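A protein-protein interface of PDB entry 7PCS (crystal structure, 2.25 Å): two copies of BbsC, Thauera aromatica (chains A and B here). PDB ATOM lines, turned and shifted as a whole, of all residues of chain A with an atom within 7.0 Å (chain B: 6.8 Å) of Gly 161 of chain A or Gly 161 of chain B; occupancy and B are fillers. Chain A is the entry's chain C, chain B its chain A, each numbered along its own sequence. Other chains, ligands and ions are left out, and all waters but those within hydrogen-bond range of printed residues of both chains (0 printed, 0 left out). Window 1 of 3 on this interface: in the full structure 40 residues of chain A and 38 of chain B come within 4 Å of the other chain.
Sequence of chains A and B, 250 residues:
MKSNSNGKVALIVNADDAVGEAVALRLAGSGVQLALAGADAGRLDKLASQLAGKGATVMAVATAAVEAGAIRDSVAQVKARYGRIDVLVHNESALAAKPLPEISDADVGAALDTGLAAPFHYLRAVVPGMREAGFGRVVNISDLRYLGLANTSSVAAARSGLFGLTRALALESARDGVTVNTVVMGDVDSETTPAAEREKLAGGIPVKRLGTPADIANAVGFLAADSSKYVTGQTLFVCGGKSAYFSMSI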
ATOM      1  N   GLY A 115      12.804 -30.819 -11.477  1.00  0.00           N
ATOM      2  CA  GLY A 115      11.382 -30.810 -11.183  1.00  0.00           C
ATOM      3  C   GLY A 115      10.864 -29.504 -10.626  1.00  0.00           C
ATOM      4  O   GLY A 115       9.681 -29.188 -10.792  1.00  0.00           O
ATOM      5  N   LEU A 116      11.727 -28.726  -9.973  1.00  0.00           N
ATOM      6  CA  LEU A 116      11.279 -27.548  -9.243  1.00  0.00           C
ATOM      7  C   LEU A 116      12.135 -26.330  -9.563  1.00  0.00           C
ATOM      8  O   LEU A 116      11.604 -25.260  -9.874  1.00  0.00           O
ATOM      9  CB  LEU A 116      11.298 -27.835  -7.744  1.00  0.00           C
ATOM     10  CG  LEU A 116      10.809 -26.740  -6.796  1.00  0.00           C
ATOM     11  CD1 LEU A 116       9.373 -26.335  -7.129  1.00  0.00           C
ATOM     12  CD2 LEU A 116      10.914 -27.198  -5.343  1.00  0.00           C
ATOM     13  N   TYR A 146       2.820 -35.348  -6.755  1.00  0.00           N
ATOM     14  CA  TYR A 146       3.008 -34.173  -5.908  1.00  0.00           C
ATOM     15  C   TYR A 146       2.246 -34.314  -4.595  1.00  0.00           C
ATOM     16  O   TYR A 146       2.632 -33.698  -3.595  1.00  0.00           O
ATOM     17  CB  TYR A 146       2.590 -32.893  -6.652  1.00  0.00           C
ATOM     18  CG  TYR A 146       1.200 -32.365  -6.347  1.00  0.00           C
ATOM     19  CD1 TYR A 146       0.940 -31.648  -5.187  1.00  0.00           C
ATOM     20  CD2 TYR A 146       0.155 -32.558  -7.238  1.00  0.00           C
ATOM     21  CE1 TYR A 146      -0.322 -31.171  -4.914  1.00  0.00           C
ATOM     22  CE2 TYR A 146      -1.105 -32.069  -6.976  1.00  0.00           C
ATOM     23  CZ  TYR A 146      -1.333 -31.379  -5.809  1.00  0.00           C
ATOM     24  OH  TYR A 146      -2.570 -30.879  -5.499  1.00  0.00           O
ATOM     25  N   SER A 153       9.053 -40.438  -2.737  1.00  0.00           N
ATOM     26  CA  SER A 153       9.383 -39.270  -1.920  1.00  0.00           C
ATOM     27  C   SER A 153      10.221 -38.255  -2.687  1.00  0.00           C
ATOM     28  O   SER A 153       9.988 -37.042  -2.587  1.00  0.00           O
ATOM     29  CB  SER A 153      10.111 -39.714  -0.649  1.00  0.00           C
ATOM     30  OG  SER A 153      11.179 -40.596  -0.954  1.00  0.00           O
ATOM     31  N   VAL A 155      10.386 -37.800  -5.941  1.00  0.00           N
ATOM     32  CA  VAL A 155       9.560 -37.129  -6.942  1.00  0.00           C
ATOM     33  C   VAL A 155       8.572 -36.177  -6.273  1.00  0.00           C
ATOM     34  O   VAL A 155       8.381 -35.039  -6.723  1.00  0.00           O
ATOM     35  CB  VAL A 155       8.830 -38.162  -7.820  1.00  0.00           C
ATOM     36  CG1 VAL A 155       8.004 -37.454  -8.886  1.00  0.00           C
ATOM     37  CG2 VAL A 155       9.819 -39.138  -8.437  1.00  0.00           C
ATOM     38  N   ALA A 156       7.934 -36.623  -5.189  1.00  0.00           N
ATOM     39  CA  ALA A 156       6.888 -35.824  -4.554  1.00  0.00           C
ATOM     40  C   ALA A 156       7.442 -34.511  -4.019  1.00  0.00           C
ATOM     41  O   ALA A 156       6.817 -33.456  -4.171  1.00  0.00           O
ATOM     42  CB  ALA A 156       6.226 -36.622  -3.432  1.00  0.00           C
ATOM     43  N   ALA A 157       8.613 -34.557  -3.383  1.00  0.00           N
ATOM     44  CA  ALA A 157       9.207 -33.337  -2.852  1.00  0.00           C
ATOM     45  C   ALA A 157       9.379 -32.291  -3.947  1.00  0.00           C
ATOM     46  O   ALA A 157       9.107 -31.105  -3.733  1.00  0.00           O
ATOM     47  CB  ALA A 157      10.555 -33.651  -2.200  1.00  0.00           C
ATOM     48  N   ALA A 158       9.833 -32.711  -5.128  1.00  0.00           N
ATOM     49  CA  ALA A 158      10.068 -31.757  -6.206  1.00  0.00           C
ATOM     50  C   ALA A 158       8.757 -31.242  -6.785  1.00  0.00           C
ATOM     51  O   ALA A 158       8.552 -30.028  -6.894  1.00  0.00           O
ATOM     52  CB  ALA A 158      10.915 -32.400  -7.304  1.00  0.00           C
ATOM     53  N   ARG A 159       7.858 -32.149  -7.174  1.00  0.00           N
ATOM     54  CA  ARG A 159       6.593 -31.718  -7.759  1.00  0.00           C
ATOM     55  C   ARG A 159       5.784 -30.895  -6.763  1.00  0.00           C
ATOM     56  O   ARG A 159       5.165 -29.891  -7.132  1.00  0.00           O
ATOM     57  CB  ARG A 159       5.779 -32.932  -8.213  1.00  0.00           C
ATOM     58  CG  ARG A 159       6.529 -33.933  -9.075  1.00  0.00           C
ATOM     59  CD  ARG A 159       6.715 -33.470 -10.513  1.00  0.00           C
ATOM     60  NE  ARG A 159       6.985 -34.606 -11.390  1.00  0.00           N
ATOM     61  CZ  ARG A 159       7.920 -34.619 -12.332  1.00  0.00           C
ATOM     62  NH1 ARG A 159       8.681 -33.563 -12.563  1.00  0.00           N
ATOM     63  NH2 ARG A 159       8.103 -35.723 -13.052  1.00  0.00           N
ATOM     64  N   SER A 160       5.756 -31.323  -5.501  1.00  0.00           N
ATOM     65  CA  SER A 160       4.955 -30.627  -4.498  1.00  0.00           C
ATOM     66  C   SER A 160       5.392 -29.179  -4.337  1.00  0.00           C
ATOM     67  O   SER A 160       4.589 -28.332  -3.933  1.00  0.00           O
ATOM     68  CB  SER A 160       5.048 -31.362  -3.162  1.00  0.00           C
ATOM     69  OG  SER A 160       4.120 -30.862  -2.214  1.00  0.00           O
ATOM     70  N   GLY A 161       6.651 -28.871  -4.652  1.00  0.00           N
ATOM     71  CA  GLY A 161       7.108 -27.498  -4.524  1.00  0.00           C
ATOM     72  C   GLY A 161       6.418 -26.557  -5.487  1.00  0.00           C
ATOM     73  O   GLY A 161       6.273 -25.364  -5.201  1.00  0.00           O
ATOM     74  N   LEU A 162       5.974 -27.076  -6.630  1.00  0.00           N
ATOM     75  CA  LEU A 162       5.299 -26.252  -7.619  1.00  0.00           C
ATOM     76  C   LEU A 162       3.945 -25.753  -7.136  1.00  0.00           C
ATOM     77  O   LEU A 162       3.459 -24.736  -7.643  1.00  0.00           O
ATOM     78  CB  LEU A 162       5.123 -27.047  -8.908  1.00  0.00           C
ATOM     79  CG  LEU A 162       6.396 -27.653  -9.503  1.00  0.00           C
ATOM     80  CD1 LEU A 162       6.057 -28.635 -10.621  1.00  0.00           C
ATOM     81  CD2 LEU A 162       7.315 -26.566 -10.014  1.00  0.00           C
ATOM     82  N   PHE A 163       3.318 -26.450  -6.186  1.00  0.00           N
ATOM     83  CA  PHE A 163       2.014 -26.025  -5.681  1.00  0.00           C
ATOM     84  C   PHE A 163       2.100 -24.645  -5.036  1.00  0.00           C
ATOM     85  O   PHE A 163       1.417 -23.703  -5.452  1.00  0.00           O
ATOM     86  CB  PHE A 163       1.478 -27.064  -4.691  1.00  0.00           C
ATOM     87  CG  PHE A 163       0.254 -26.618  -3.946  1.00  0.00           C
ATOM     88  CD1 PHE A 163      -0.962 -26.528  -4.589  1.00  0.00           C
ATOM     89  CD2 PHE A 163       0.320 -26.307  -2.596  1.00  0.00           C
ATOM     90  CE1 PHE A 163      -2.101 -26.119  -3.906  1.00  0.00           C
ATOM     91  CE2 PHE A 163      -0.810 -25.898  -1.908  1.00  0.00           C
ATOM     92  CZ  PHE A 163      -2.024 -25.805  -2.568  1.00  0.00           C
ATOM     93  N   GLY A 164       2.935 -24.505  -4.008  1.00  0.00           N
ATOM     94  CA  GLY A 164       3.115 -23.201  -3.392  1.00  0.00           C
ATOM     95  C   GLY A 164       3.773 -22.202  -4.325  1.00  0.00           C
ATOM     96  O   GLY A 164       3.451 -21.012  -4.300  1.00  0.00           O
ATOM     97  N   LEU A 165       4.700 -22.671  -5.166  1.00  0.00           N
ATOM     98  CA  LEU A 165       5.390 -21.774  -6.088  1.00  0.00           C
ATOM     99  C   LEU A 165       4.411 -21.119  -7.055  1.00  0.00           C
ATOM    100  O   LEU A 165       4.397 -19.891  -7.212  1.00  0.00           O
ATOM    101  CB  LEU A 165       6.467 -22.543  -6.852  1.00  0.00           C
ATOM    102  CG  LEU A 165       7.153 -21.790  -7.990  1.00  0.00           C
ATOM    103  CD1 LEU A 165       7.778 -20.491  -7.498  1.00  0.00           C
ATOM    104  CD2 LEU A 165       8.220 -22.668  -8.649  1.00  0.00           C
ATOM    105  N   THR A 166       3.583 -21.929  -7.721  1.00  0.00           N
ATOM    106  CA  THR A 166       2.638 -21.381  -8.687  1.00  0.00           C
ATOM    107  C   THR A 166       1.678 -20.405  -8.019  1.00  0.00           C
ATOM    108  O   THR A 166       1.400 -19.327  -8.559  1.00  0.00           O
ATOM    109  CB  THR A 166       1.856 -22.504  -9.369  1.00  0.00           C
ATOM    110  OG1 THR A 166       1.257 -23.342  -8.377  1.00  0.00           O
ATOM    111  CG2 THR A 166       2.765 -23.337 -10.240  1.00  0.00           C
ATOM    112  N   LEU B 116      14.078 -27.472   2.138  1.00  0.00           N
ATOM    113  CA  LEU B 116      13.485 -28.700   1.624  1.00  0.00           C
ATOM    114  C   LEU B 116      14.461 -29.866   1.592  1.00  0.00           C
ATOM    115  O   LEU B 116      14.148 -30.949   2.098  1.00  0.00           O
ATOM    116  CB  LEU B 116      12.935 -28.444   0.225  1.00  0.00           C
ATOM    117  CG  LEU B 116      12.258 -29.598  -0.507  1.00  0.00           C
ATOM    118  CD1 LEU B 116      11.114 -30.146   0.293  1.00  0.00           C
ATOM    119  CD2 LEU B 116      11.788 -29.127  -1.884  1.00  0.00           C
ATOM    120  N   TYR B 146       3.887 -21.977   2.672  1.00  0.00           N
ATOM    121  CA  TYR B 146       3.917 -23.127   1.769  1.00  0.00           C
ATOM    122  C   TYR B 146       2.727 -23.111   0.816  1.00  0.00           C
ATOM    123  O   TYR B 146       2.809 -23.670  -0.284  1.00  0.00           O
ATOM    124  CB  TYR B 146       3.969 -24.442   2.567  1.00  0.00           C
ATOM    125  CG  TYR B 146       2.651 -25.184   2.686  1.00  0.00           C
ATOM    126  CD1 TYR B 146       2.198 -26.007   1.664  1.00  0.00           C
ATOM    127  CD2 TYR B 146       1.868 -25.069   3.823  1.00  0.00           C
ATOM    128  CE1 TYR B 146       0.994 -26.672   1.761  1.00  0.00           C
ATOM    129  CE2 TYR B 146       0.658 -25.740   3.933  1.00  0.00           C
ATOM    130  CZ  TYR B 146       0.234 -26.543   2.900  1.00  0.00           C
ATOM    131  OH  TYR B 146      -0.961 -27.215   3.006  1.00  0.00           O
ATOM    132  N   SER B 153       7.869 -16.469  -3.202  1.00  0.00           N
ATOM    133  CA  SER B 153       7.980 -17.598  -4.122  1.00  0.00           C
ATOM    134  C   SER B 153       9.099 -18.556  -3.736  1.00  0.00           C
ATOM    135  O   SER B 153       8.908 -19.778  -3.755  1.00  0.00           O
ATOM    136  CB  SER B 153       8.192 -17.081  -5.545  1.00  0.00           C
ATOM    137  OG  SER B 153       9.226 -16.111  -5.580  1.00  0.00           O
ATOM    138  N   VAL B 155      10.453 -18.989  -0.783  1.00  0.00           N
ATOM    139  CA  VAL B 155      10.057 -19.686   0.437  1.00  0.00           C
ATOM    140  C   VAL B 155       8.943 -20.675   0.137  1.00  0.00           C
ATOM    141  O   VAL B 155       8.958 -21.816   0.617  1.00  0.00           O
ATOM    142  CB  VAL B 155       9.636 -18.677   1.521  1.00  0.00           C
ATOM    143  CG1 VAL B 155       9.217 -19.408   2.794  1.00  0.00           C
ATOM    144  CG2 VAL B 155      10.777 -17.702   1.809  1.00  0.00           C
ATOM    145  N   ALA B 156       7.956 -20.256  -0.660  1.00  0.00           N
ATOM    146  CA  ALA B 156       6.819 -21.125  -0.937  1.00  0.00           C
ATOM    147  C   ALA B 156       7.264 -22.389  -1.663  1.00  0.00           C
ATOM    148  O   ALA B 156       6.819 -23.494  -1.332  1.00  0.00           O
ATOM    149  CB  ALA B 156       5.762 -20.376  -1.757  1.00  0.00           C
ATOM    150  N   ALA B 157       8.139 -22.250  -2.658  1.00  0.00           N
ATOM    151  CA  ALA B 157       8.616 -23.420  -3.383  1.00  0.00           C
ATOM    152  C   ALA B 157       9.271 -24.424  -2.446  1.00  0.00           C
ATOM    153  O   ALA B 157       9.024 -25.631  -2.546  1.00  0.00           O
ATOM    154  CB  ALA B 157       9.596 -22.991  -4.473  1.00  0.00           C
ATOM    155  N   ALA B 158      10.100 -23.944  -1.515  1.00  0.00           N
ATOM    156  CA  ALA B 158      10.814 -24.850  -0.623  1.00  0.00           C
ATOM    157  C   ALA B 158       9.868 -25.492   0.384  1.00  0.00           C
ATOM    158  O   ALA B 158       9.854 -26.717   0.546  1.00  0.00           O
ATOM    159  CB  ALA B 158      11.932 -24.098   0.098  1.00  0.00           C
ATOM    160  N   ARG B 159       9.080 -24.675   1.087  1.00  0.00           N
ATOM    161  CA  ARG B 159       8.171 -25.229   2.083  1.00  0.00           C
ATOM    162  C   ARG B 159       7.132 -26.138   1.439  1.00  0.00           C
ATOM    163  O   ARG B 159       6.805 -27.199   1.983  1.00  0.00           O
ATOM    164  CB  ARG B 159       7.480 -24.106   2.856  1.00  0.00           C
ATOM    165  CG  ARG B 159       8.405 -23.050   3.444  1.00  0.00           C
ATOM    166  CD  ARG B 159       9.142 -23.548   4.686  1.00  0.00           C
ATOM    167  NE  ARG B 159       9.591 -22.436   5.518  1.00  0.00           N
ATOM    168  CZ  ARG B 159      10.804 -22.327   6.042  1.00  0.00           C
ATOM    169  NH1 ARG B 159      11.726 -23.259   5.854  1.00  0.00           N
ATOM    170  NH2 ARG B 159      11.099 -21.258   6.779  1.00  0.00           N
ATOM    171  N   SER B 160       6.595 -25.729   0.284  1.00  0.00           N
ATOM    172  CA  SER B 160       5.536 -26.495  -0.368  1.00  0.00           C
ATOM    173  C   SER B 160       5.983 -27.912  -0.700  1.00  0.00           C
ATOM    174  O   SER B 160       5.144 -28.813  -0.827  1.00  0.00           O
ATOM    175  CB  SER B 160       5.077 -25.779  -1.639  1.00  0.00           C
ATOM    176  OG  SER B 160       3.907 -26.379  -2.159  1.00  0.00           O
ATOM    177  N   GLY B 161       7.293 -28.122  -0.860  1.00  0.00           N
ATOM    178  CA  GLY B 161       7.794 -29.455  -1.148  1.00  0.00           C
ATOM    179  C   GLY B 161       7.592 -30.428  -0.004  1.00  0.00           C
ATOM    180  O   GLY B 161       7.493 -31.640  -0.222  1.00  0.00           O
ATOM    181  N   LEU B 162       7.531 -29.917   1.223  1.00  0.00           N
ATOM    182  CA  LEU B 162       7.345 -30.772   2.386  1.00  0.00           C
ATOM    183  C   LEU B 162       5.971 -31.423   2.414  1.00  0.00           C
ATOM    184  O   LEU B 162       5.808 -32.458   3.066  1.00  0.00           O
ATOM    185  CB  LEU B 162       7.558 -29.958   3.660  1.00  0.00           C
ATOM    186  CG  LEU B 162       8.893 -29.218   3.739  1.00  0.00           C
ATOM    187  CD1 LEU B 162       8.891 -28.232   4.902  1.00  0.00           C
ATOM    188  CD2 LEU B 162      10.032 -30.201   3.884  1.00  0.00           C
ATOM    189  N   PHE B 163       4.983 -30.836   1.740  1.00  0.00           N
ATOM    190  CA  PHE B 163       3.638 -31.396   1.739  1.00  0.00           C
ATOM    191  C   PHE B 163       3.630 -32.798   1.141  1.00  0.00           C
ATOM    192  O   PHE B 163       3.260 -33.771   1.806  1.00  0.00           O
ATOM    193  CB  PHE B 163       2.702 -30.471   0.959  1.00  0.00           C
ATOM    194  CG  PHE B 163       1.339 -31.058   0.701  1.00  0.00           C
ATOM    195  CD1 PHE B 163       0.411 -31.169   1.723  1.00  0.00           C
ATOM    196  CD2 PHE B 163       0.986 -31.499  -0.566  1.00  0.00           C
ATOM    197  CE1 PHE B 163      -0.846 -31.711   1.479  1.00  0.00           C
ATOM    198  CE2 PHE B 163      -0.255 -32.045  -0.804  1.00  0.00           C
ATOM    199  CZ  PHE B 163      -1.166 -32.154   0.218  1.00  0.00           C
ATOM    200  N   GLY B 164       4.048 -32.917  -0.119  1.00  0.00           N
ATOM    201  CA  GLY B 164       4.107 -34.227  -0.747  1.00  0.00           C
ATOM    202  C   GLY B 164       5.146 -35.138  -0.121  1.00  0.00           C
ATOM    203  O   GLY B 164       4.940 -36.350  -0.014  1.00  0.00           O
ATOM    204  N   LEU B 165       6.273 -34.570   0.306  1.00  0.00           N
ATOM    205  CA  LEU B 165       7.326 -35.387   0.898  1.00  0.00           C
ATOM    206  C   LEU B 165       6.830 -36.095   2.151  1.00  0.00           C
ATOM    207  O   LEU B 165       6.997 -37.311   2.298  1.00  0.00           O
ATOM    208  CB  LEU B 165       8.537 -34.520   1.217  1.00  0.00           C
ATOM    209  CG  LEU B 165       9.648 -35.218   1.997  1.00  0.00           C
ATOM    210  CD1 LEU B 165      10.153 -36.453   1.257  1.00  0.00           C
ATOM    211  CD2 LEU B 165      10.791 -34.246   2.273  1.00  0.00           C
ATOM    212  N   THR B 166       6.235 -35.342   3.082  1.00  0.00           N
ATOM    213  CA  THR B 166       5.764 -35.960   4.316  1.00  0.00           C
ATOM    214  C   THR B 166       4.729 -37.039   4.023  1.00  0.00           C
ATOM    215  O   THR B 166       4.810 -38.152   4.556  1.00  0.00           O
ATOM    216  CB  THR B 166       5.189 -34.907   5.265  1.00  0.00           C
ATOM    217  OG1 THR B 166       4.215 -34.114   4.582  1.00  0.00           O
ATOM    218  CG2 THR B 166       6.287 -34.008   5.796  1.00  0.00           C
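Ala 156 of chain A touches Gly 164 of chain B, and with the chains exchanged Gly 164 of chain A touches Ala 156 of chain B.
Ala 157 of chain A touches Gly 161 of chain B, and with the chains exchanged Gly 161 of chain A touches Ala 157 of chain B.
Ser 160 of chain A touches its own counterpart, Ser 160 of chain B.
Ser 160 of chain A touches Phe 163 of chain B, and with the chains exchanged Phe 163 of chain A touches Ser 160 of chain B.
15 positions are printed for both chains.
Of the 15 printed residues of chain B, 10 touch a printed residue of chain A.
Hydrophobic or aromatic side chains of chain B that line the printed part of chain A: Leu 116, Ala 156, Ala 157, Phe 163 and Leu 165.
Along chain B the printed residues that touch a printed residue of chain A span positions 116 to 165.
Hydrophobic or aromatic side chains of chain A within 4 Å of the printed part of chain B: Leu 116, Ala 156, Phe 163 and Leu 165.
Among the printed residues, no Asp or Glu carboxylate lies within 4 Å of a Lys or Arg side-chain nitrogen of the other chain.
OG of Ser 160 of chain A is in hydrogen-bond range of N of Gly 164 of chain B.
O of Ser 160 of chain B is in hydrogen-bond range of OG of Ser 160 of chain A (2.7 Å).
The side-chain hydroxyl (OG) of Ser 160 of chain B lies within hydrogen-bond range of the backbone NH (N) of Gly 164 of chain A, at 2.8 Å.
The backbone carbonyl oxygen (O) of Tyr 146 of chain A lies close to the side-chain hydroxyl (OG) of Ser 160 of chain A (3.5 Å).
The backbone carbonyl oxygen (O) of Phe 163 of chain A lies within hydrogen-bond range of the side-chain hydroxyl (OG1) of Thr 166 of chain A (3.0 Å).
The side-chain hydroxyl of Thr 166 of chain B is in hydrogen-bond range of the backbone carbonyl oxygen of Phe 163 of chain B (3.0 Å).
The backbone carbonyl oxygen (O) of Tyr 146 of chain B sits close to the side-chain hydroxyl (OG) of Ser 160 of chain B (3.5 Å).
O of Tyr 146 of chain A touches CA of Gly 164 of chain B, 3.3 Å away.
CB of Ser 153 of chain A touches CD1 of Leu 165 of chain B, at 3.8 Å.
Ala 156 of chain A touches Gly 164 of chain B (CB to O, 3.7 Å).
Ser 160 of chain A touches Gly 161 of chain B.
O of Ala 157 of chain B touches CA of Gly 161 of chain A, at 3.3 Å.
Gly 161 of chain A touches Ser 160 of chain B (O to CB, 3.8 Å).
Gly 161 of chain A touches Gly 161 of chain B.
Phe 163 of chain A touches Ser 160 of chain B.
Leu 165 of chain A touches Ser 153 of chain B.
Ala 157 of chain B touches Leu 165 of chain A (CB to CB, 3.96 Å).
Gly 161 of chain A touches just these residues of chain B: Ala 157 (3.3 Å), Ser 160 (3.8 Å) and Gly 161 (3.7 Å).
Of chain A, only Ala 157 (3.3 Å), Ser 160 (3.8 Å) and Gly 161 (3.7 Å) come within 4 Å of Gly 161 of chain B.
Of the printed residues of chain B, Ala 156 of chain A touches Gly 164.
Of the printed residues of chain B, Tyr 146 of chain A touches Gly 164 (3.3 Å).
Of the printed residues of chain B, Leu 165 of chain A touches Ser 153 (3.95 Å) and Ala 157 (3.96 Å).
Of the printed residues of chain A, Ser 160 of chain B touches Ser 160, Gly 161, Phe 163 and Gly 164.
Val 155 of chain B touches none of the printed residues of chain A.
Ala 158 of chain A touches none of the printed residues of chain B.
The nearest residue of chain B that does not touch Gly 161 of chain A is Ala 156 of chain B (4.3 Å).
The nearest residue of chain A that does not touch Gly 161 of chain B is Ala 156 of chain A (4.4 Å).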
